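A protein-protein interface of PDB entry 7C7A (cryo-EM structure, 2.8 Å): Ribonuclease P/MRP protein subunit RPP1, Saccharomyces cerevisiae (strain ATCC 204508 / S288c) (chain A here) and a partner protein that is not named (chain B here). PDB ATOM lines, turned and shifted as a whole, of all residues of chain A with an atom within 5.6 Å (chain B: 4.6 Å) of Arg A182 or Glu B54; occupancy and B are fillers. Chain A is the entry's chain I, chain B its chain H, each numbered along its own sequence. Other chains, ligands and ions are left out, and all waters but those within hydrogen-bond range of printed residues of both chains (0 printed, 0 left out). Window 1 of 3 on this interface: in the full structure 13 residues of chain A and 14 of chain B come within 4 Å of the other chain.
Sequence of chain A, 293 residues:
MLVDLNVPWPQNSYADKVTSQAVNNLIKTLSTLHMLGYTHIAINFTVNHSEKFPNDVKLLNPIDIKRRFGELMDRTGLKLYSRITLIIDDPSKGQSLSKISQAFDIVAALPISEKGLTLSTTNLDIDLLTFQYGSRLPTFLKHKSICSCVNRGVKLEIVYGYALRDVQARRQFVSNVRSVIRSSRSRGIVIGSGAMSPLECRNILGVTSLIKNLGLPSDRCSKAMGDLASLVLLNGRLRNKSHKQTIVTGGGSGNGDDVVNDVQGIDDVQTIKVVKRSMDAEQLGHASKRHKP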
ATOM      1  N   PHE A 140     -15.546   3.441  26.336  1.00  0.00           N
ATOM      2  CA  PHE A 140     -15.202   2.884  25.028  1.00  0.00           C
ATOM      3  C   PHE A 140     -13.865   3.483  24.614  1.00  0.00           C
ATOM      4  O   PHE A 140     -13.686   4.702  24.697  1.00  0.00           O
ATOM      5  CB  PHE A 140     -16.287   3.186  23.996  1.00  0.00           C
ATOM      6  CG  PHE A 140     -16.132   2.422  22.707  1.00  0.00           C
ATOM      7  CD1 PHE A 140     -16.386   1.061  22.658  1.00  0.00           C
ATOM      8  CD2 PHE A 140     -15.752   3.068  21.541  1.00  0.00           C
ATOM      9  CE1 PHE A 140     -16.255   0.356  21.476  1.00  0.00           C
ATOM     10  CE2 PHE A 140     -15.620   2.368  20.353  1.00  0.00           C
ATOM     11  CZ  PHE A 140     -15.873   1.010  20.322  1.00  0.00           C
ATOM     12  N   LEU A 141     -12.936   2.639  24.179  1.00  0.00           N
ATOM     13  CA  LEU A 141     -11.676   3.142  23.653  1.00  0.00           C
ATOM     14  C   LEU A 141     -11.791   3.418  22.160  1.00  0.00           C
ATOM     15  O   LEU A 141     -12.092   2.521  21.368  1.00  0.00           O
ATOM     16  CB  LEU A 141     -10.543   2.156  23.933  1.00  0.00           C
ATOM     17  CG  LEU A 141      -9.774   2.400  25.236  1.00  0.00           C
ATOM     18  CD1 LEU A 141      -9.030   3.720  25.149  1.00  0.00           C
ATOM     19  CD2 LEU A 141     -10.687   2.395  26.451  1.00  0.00           C
ATOM     20  N   VAL A 177      -8.234  -6.341  26.351  1.00  0.00           N
ATOM     21  CA  VAL A 177      -6.943  -6.334  25.672  1.00  0.00           C
ATOM     22  C   VAL A 177      -7.130  -6.368  24.159  1.00  0.00           C
ATOM     23  O   VAL A 177      -6.417  -5.678  23.424  1.00  0.00           O
ATOM     24  CB  VAL A 177      -6.052  -7.490  26.172  1.00  0.00           C
ATOM     25  CG1 VAL A 177      -6.630  -8.842  25.801  1.00  0.00           C
ATOM     26  CG2 VAL A 177      -4.642  -7.346  25.621  1.00  0.00           C
ATOM     27  N   ARG A 178      -8.109  -7.131  23.663  1.00  0.00           N
ATOM     28  CA  ARG A 178      -8.376  -7.101  22.230  1.00  0.00           C
ATOM     29  C   ARG A 178      -8.900  -5.739  21.792  1.00  0.00           C
ATOM     30  O   ARG A 178      -8.527  -5.247  20.721  1.00  0.00           O
ATOM     31  CB  ARG A 178      -9.359  -8.206  21.849  1.00  0.00           C
ATOM     32  CG  ARG A 178      -8.685  -9.514  21.478  1.00  0.00           C
ATOM     33  CD  ARG A 178      -9.654 -10.679  21.523  1.00  0.00           C
ATOM     34  NE  ARG A 178      -9.013 -11.892  22.017  1.00  0.00           N
ATOM     35  CZ  ARG A 178      -9.495 -13.119  21.843  1.00  0.00           C
ATOM     36  NH1 ARG A 178      -8.839 -14.160  22.333  1.00  0.00           N
ATOM     37  NH2 ARG A 178     -10.631 -13.303  21.184  1.00  0.00           N
ATOM     38  N   SER A 179      -9.741  -5.108  22.615  1.00  0.00           N
ATOM     39  CA  SER A 179     -10.226  -3.768  22.300  1.00  0.00           C
ATOM     40  C   SER A 179      -9.079  -2.767  22.222  1.00  0.00           C
ATOM     41  O   SER A 179      -9.009  -1.969  21.279  1.00  0.00           O
ATOM     42  CB  SER A 179     -11.256  -3.326  23.338  1.00  0.00           C
ATOM     43  OG  SER A 179     -11.716  -2.011  23.076  1.00  0.00           O
ATOM     44  N   VAL A 180      -8.167  -2.795  23.198  1.00  0.00           N
ATOM     45  CA  VAL A 180      -7.089  -1.810  23.215  1.00  0.00           C
ATOM     46  C   VAL A 180      -6.073  -2.107  22.116  1.00  0.00           C
ATOM     47  O   VAL A 180      -5.418  -1.195  21.599  1.00  0.00           O
ATOM     48  CB  VAL A 180      -6.430  -1.747  24.608  1.00  0.00           C
ATOM     49  CG1 VAL A 180      -5.600  -2.988  24.879  1.00  0.00           C
ATOM     50  CG2 VAL A 180      -5.585  -0.485  24.746  1.00  0.00           C
ATOM     51  N   ILE A 181      -5.946  -3.375  21.716  1.00  0.00           N
ATOM     52  CA  ILE A 181      -5.060  -3.702  20.604  1.00  0.00           C
ATOM     53  C   ILE A 181      -5.659  -3.218  19.291  1.00  0.00           C
ATOM     54  O   ILE A 181      -4.950  -2.697  18.420  1.00  0.00           O
ATOM     55  CB  ILE A 181      -4.773  -5.216  20.577  1.00  0.00           C
ATOM     56  CG1 ILE A 181      -3.749  -5.585  21.654  1.00  0.00           C
ATOM     57  CG2 ILE A 181      -4.281  -5.649  19.205  1.00  0.00           C
ATOM     58  CD1 ILE A 181      -3.332  -7.039  21.632  1.00  0.00           C
ATOM     59  N   ARG A 182      -6.975  -3.366  19.132  1.00  0.00           N
ATOM     60  CA  ARG A 182      -7.647  -2.878  17.937  1.00  0.00           C
ATOM     61  C   ARG A 182      -7.626  -1.357  17.854  1.00  0.00           C
ATOM     62  O   ARG A 182      -7.503  -0.803  16.756  1.00  0.00           O
ATOM     63  CB  ARG A 182      -9.087  -3.397  17.908  1.00  0.00           C
ATOM     64  CG  ARG A 182      -9.843  -3.135  16.617  1.00  0.00           C
ATOM     65  CD  ARG A 182     -10.769  -1.936  16.758  1.00  0.00           C
ATOM     66  NE  ARG A 182     -11.560  -1.996  17.985  1.00  0.00           N
ATOM     67  CZ  ARG A 182     -12.305  -0.994  18.440  1.00  0.00           C
ATOM     68  NH1 ARG A 182     -12.991  -1.136  19.566  1.00  0.00           N
ATOM     69  NH2 ARG A 182     -12.363   0.150  17.771  1.00  0.00           N
ATOM     70  N   SER A 183      -7.738  -0.671  18.990  1.00  0.00           N
ATOM     71  CA  SER A 183      -7.757   0.786  18.996  1.00  0.00           C
ATOM     72  C   SER A 183      -6.364   1.397  18.867  1.00  0.00           C
ATOM     73  O   SER A 183      -6.193   2.399  18.162  1.00  0.00           O
ATOM     74  CB  SER A 183      -8.428   1.296  20.273  1.00  0.00           C
ATOM     75  OG  SER A 183      -8.217   2.687  20.441  1.00  0.00           O
ATOM     76  N   SER A 184      -5.362   0.818  19.533  1.00  0.00           N
ATOM     77  CA  SER A 184      -4.024   1.404  19.521  1.00  0.00           C
ATOM     78  C   SER A 184      -3.342   1.211  18.172  1.00  0.00           C
ATOM     79  O   SER A 184      -2.318   1.846  17.893  1.00  0.00           O
ATOM     80  CB  SER A 184      -3.177   0.803  20.643  1.00  0.00           C
ATOM     81  OG  SER A 184      -2.914  -0.573  20.414  1.00  0.00           O
ATOM     82  N   ARG A 185      -3.884   0.331  17.330  1.00  0.00           N
ATOM     83  CA  ARG A 185      -3.339  -0.043  16.025  1.00  0.00           C
ATOM     84  C   ARG A 185      -1.972  -0.701  16.161  1.00  0.00           C
ATOM     85  O   ARG A 185      -1.195  -0.702  15.191  1.00  0.00           O
ATOM     86  CB  ARG A 185      -3.252   1.148  15.063  1.00  0.00           C
ATOM     87  CG  ARG A 185      -4.610   1.645  14.599  1.00  0.00           C
ATOM     88  CD  ARG A 185      -4.503   2.905  13.757  1.00  0.00           C
ATOM     89  NE  ARG A 185      -5.817   3.441  13.413  1.00  0.00           N
ATOM     90  CZ  ARG A 185      -6.417   3.262  12.241  1.00  0.00           C
ATOM     91  NH1 ARG A 185      -5.819   2.560  11.289  1.00  0.00           N
ATOM     92  NH2 ARG A 185      -7.615   3.787  12.018  1.00  0.00           N
ATOM     93  N   PHE B   6      -5.415   0.223   6.738  1.00  0.00           N
ATOM     94  CA  PHE B   6      -5.781  -0.637   7.855  1.00  0.00           C
ATOM     95  C   PHE B   6      -7.294  -0.622   8.036  1.00  0.00           C
ATOM     96  O   PHE B   6      -7.891   0.439   8.247  1.00  0.00           O
ATOM     97  CB  PHE B   6      -5.077  -0.180   9.131  1.00  0.00           C
ATOM     98  CG  PHE B   6      -5.405  -1.012  10.339  1.00  0.00           C
ATOM     99  CD1 PHE B   6      -4.726  -2.193  10.588  1.00  0.00           C
ATOM    100  CD2 PHE B   6      -6.389  -0.611  11.230  1.00  0.00           C
ATOM    101  CE1 PHE B   6      -5.025  -2.961  11.697  1.00  0.00           C
ATOM    102  CE2 PHE B   6      -6.692  -1.374  12.341  1.00  0.00           C
ATOM    103  CZ  PHE B   6      -6.009  -2.551  12.575  1.00  0.00           C
ATOM    104  N   GLU B   8     -10.617  -1.064  10.026  1.00  0.00           N
ATOM    105  CA  GLU B   8     -11.010  -0.992  11.429  1.00  0.00           C
ATOM    106  C   GLU B   8     -11.713  -2.275  11.858  1.00  0.00           C
ATOM    107  O   GLU B   8     -11.273  -2.964  12.785  1.00  0.00           O
ATOM    108  CB  GLU B   8     -11.906   0.227  11.654  1.00  0.00           C
ATOM    109  CG  GLU B   8     -12.226   0.516  13.108  1.00  0.00           C
ATOM    110  CD  GLU B   8     -11.012   0.984  13.887  1.00  0.00           C
ATOM    111  OE1 GLU B   8     -10.083   1.546  13.268  1.00  0.00           O
ATOM    112  OE2 GLU B   8     -10.986   0.798  15.121  1.00  0.00           O
ATOM    113  N   TRP B   9     -12.809  -2.611  11.188  1.00  0.00           N
ATOM    114  CA  TRP B   9     -13.503  -3.877  11.402  1.00  0.00           C
ATOM    115  C   TRP B   9     -14.159  -4.275  10.084  1.00  0.00           C
ATOM    116  O   TRP B   9     -13.835  -3.743   9.016  1.00  0.00           O
ATOM    117  CB  TRP B   9     -14.504  -3.770  12.565  1.00  0.00           C
ATOM    118  CG  TRP B   9     -15.442  -2.610  12.469  1.00  0.00           C
ATOM    119  CD1 TRP B   9     -16.377  -2.385  11.500  1.00  0.00           C
ATOM    120  CD2 TRP B   9     -15.558  -1.525  13.397  1.00  0.00           C
ATOM    121  NE1 TRP B   9     -17.055  -1.218  11.758  1.00  0.00           N
ATOM    122  CE2 TRP B   9     -16.572  -0.673  12.919  1.00  0.00           C
ATOM    123  CE3 TRP B   9     -14.898  -1.190  14.583  1.00  0.00           C
ATOM    124  CZ2 TRP B   9     -16.941   0.493  13.583  1.00  0.00           C
ATOM    125  CZ3 TRP B   9     -15.266  -0.030  15.241  1.00  0.00           C
ATOM    126  CH2 TRP B   9     -16.277   0.797  14.740  1.00  0.00           C
ATOM    127  N   GLY B  52     -13.899 -13.440  24.033  1.00  0.00           N
ATOM    128  CA  GLY B  52     -13.337 -12.103  24.045  1.00  0.00           C
ATOM    129  C   GLY B  52     -13.423 -11.386  22.713  1.00  0.00           C
ATOM    130  O   GLY B  52     -12.731 -10.387  22.496  1.00  0.00           O
ATOM    131  N   VAL B  53     -14.272 -11.880  21.813  1.00  0.00           N
ATOM    132  CA  VAL B  53     -14.418 -11.262  20.501  1.00  0.00           C
ATOM    133  C   VAL B  53     -15.320 -10.040  20.617  1.00  0.00           C
ATOM    134  O   VAL B  53     -16.396 -10.097  21.225  1.00  0.00           O
ATOM    135  CB  VAL B  53     -14.970 -12.274  19.487  1.00  0.00           C
ATOM    136  CG1 VAL B  53     -15.382 -11.575  18.199  1.00  0.00           C
ATOM    137  CG2 VAL B  53     -13.938 -13.356  19.203  1.00  0.00           C
ATOM    138  N   GLU B  54     -14.878  -8.925  20.039  1.00  0.00           N
ATOM    139  CA  GLU B  54     -15.643  -7.684  20.084  1.00  0.00           C
ATOM    140  C   GLU B  54     -16.709  -7.692  18.994  1.00  0.00           C
ATOM    141  O   GLU B  54     -16.409  -7.968  17.828  1.00  0.00           O
ATOM    142  CB  GLU B  54     -14.716  -6.480  19.921  1.00  0.00           C
ATOM    143  CG  GLU B  54     -15.425  -5.137  20.003  1.00  0.00           C
ATOM    144  CD  GLU B  54     -14.473  -3.967  19.852  1.00  0.00           C
ATOM    145  OE1 GLU B  54     -13.261  -4.206  19.670  1.00  0.00           O
ATOM    146  OE2 GLU B  54     -14.938  -2.809  19.913  1.00  0.00           O
ATOM    147  N   TYR B  55     -17.949  -7.386  19.374  1.00  0.00           N
ATOM    148  CA  TYR B  55     -19.061  -7.312  18.439  1.00  0.00           C
ATOM    149  C   TYR B  55     -20.163  -6.447  19.033  1.00  0.00           C
ATOM    150  O   TYR B  55     -20.417  -6.495  20.240  1.00  0.00           O
ATOM    151  CB  TYR B  55     -19.608  -8.708  18.099  1.00  0.00           C
ATOM    152  CG  TYR B  55     -20.121  -9.487  19.292  1.00  0.00           C
ATOM    153  CD1 TYR B  55     -19.268 -10.285  20.044  1.00  0.00           C
ATOM    154  CD2 TYR B  55     -21.460  -9.434  19.660  1.00  0.00           C
ATOM    155  CE1 TYR B  55     -19.733 -11.001  21.136  1.00  0.00           C
ATOM    156  CE2 TYR B  55     -21.933 -10.145  20.749  1.00  0.00           C
ATOM    157  CZ  TYR B  55     -21.067 -10.927  21.482  1.00  0.00           C
ATOM    158  OH  TYR B  55     -21.538 -11.635  22.565  1.00  0.00           O
ATOM    159  N   ARG B  68     -20.712  -6.093  13.302  1.00  0.00           N
ATOM    160  CA  ARG B  68     -19.386  -5.647  12.898  1.00  0.00           C
ATOM    161  C   ARG B  68     -18.332  -6.366  13.734  1.00  0.00           C
ATOM    162  O   ARG B  68     -18.388  -6.348  14.969  1.00  0.00           O
ATOM    163  CB  ARG B  68     -19.254  -4.130  13.050  1.00  0.00           C
ATOM    164  CG  ARG B  68     -19.724  -3.595  14.394  1.00  0.00           C
ATOM    165  CD  ARG B  68     -19.572  -2.086  14.486  1.00  0.00           C
ATOM    166  NE  ARG B  68     -19.852  -1.603  15.836  1.00  0.00           N
ATOM    167  CZ  ARG B  68     -19.880  -0.320  16.183  1.00  0.00           C
ATOM    168  NH1 ARG B  68     -19.651   0.622  15.278  1.00  0.00           N
ATOM    169  NH2 ARG B  68     -20.141   0.022  17.437  1.00  0.00           N
ATOM    170  N   VAL B  69     -17.384  -7.011  13.060  1.00  0.00           N
ATOM    171  CA  VAL B  69     -16.321  -7.764  13.712  1.00  0.00           C
ATOM    172  C   VAL B  69     -14.986  -7.262  13.180  1.00  0.00           C
ATOM    173  O   VAL B  69     -14.872  -6.916  11.999  1.00  0.00           O
ATOM    174  CB  VAL B  69     -16.471  -9.283  13.480  1.00  0.00           C
ATOM    175  CG1 VAL B  69     -15.421 -10.060  14.264  1.00  0.00           C
ATOM    176  CG2 VAL B  69     -17.871  -9.746  13.853  1.00  0.00           C
ATOM    177  N   ASN B  70     -13.984  -7.214  14.057  1.00  0.00           N
ATOM    178  CA  ASN B  70     -12.659  -6.748  13.671  1.00  0.00           C
ATOM    179  C   ASN B  70     -12.106  -7.582  12.521  1.00  0.00           C
ATOM    180  O   ASN B  70     -12.412  -8.769  12.378  1.00  0.00           O
ATOM    181  CB  ASN B  70     -11.707  -6.804  14.867  1.00  0.00           C
ATOM    182  CG  ASN B  70     -12.104  -5.847  15.975  1.00  0.00           C
ATOM    183  OD1 ASN B  70     -12.679  -4.789  15.721  1.00  0.00           O
ATOM    184  ND2 ASN B  70     -11.800  -6.218  17.214  1.00  0.00           N
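The side-chain carboxylate of Glu B8 lies within salt-bridge range of the guanidinium group of Arg A182, 3.1 Å away. OE1 of Glu B8 is in salt-bridge range of NH2 of Arg A185 (3.6 Å). The guanidinium group (NH1) of Arg A182 is in salt-bridge range of the side-chain carboxylate (OE2) of Glu B54 (2.6 Å).
The side-chain amide nitrogen of Asn B70 sits at hydrogen-bond distance from the side-chain carboxylate of Glu B54, at 3.5 Å.
Glu B54 touches Phe A140. Arg A178 touches Gly B52. Val B53 touches Arg A178 (CG2 to NH2, 3.9 Å). Trp B9 touches Arg A182 (CZ3 to NH2, 3.9 Å). Arg A182 touches Asn B70. NH1 of Arg A185 touches CD2 of Phe B6, 3.2 Å away.
Arg A182 touches just these residues of chain B: Glu B8, Trp B9, Glu B54 and Asn B70. Glu B54 touches just these residues of chain A: Phe A140 and Arg A182. Of the printed residues of chain B, Arg A178 touches Gly B52 and Val B53. Of the printed residues of chain A, Phe B6 touches Arg A185 (3.2 Å). Printed residues of chain A within 4 Å of Glu B8: Arg A182 (3.1 Å) and Arg A185 (3.6 Å). Of the printed residues of chain A, Asn B70 touches Arg A182. Of the printed residues of chain A, Trp B9 touches Arg A182 (3.9 Å). The nearest residue of chain B that does not touch Arg A182 is Phe B6 (4.5 Å).
Hydrophobic or aromatic side chains of chain A that line the printed part of chain B: Phe A140. Among the printed residues, 9 pairs touch across the chains. Among the printed residues, Asp or Glu carboxylates within 4 Å of a Lys or Arg side-chain nitrogen of the other chain: Arg A182 with Glu B8 (3.1 Å), Arg A182 with Glu B54 (2.6 Å) and Arg A185 with Glu B8 (3.6 Å).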
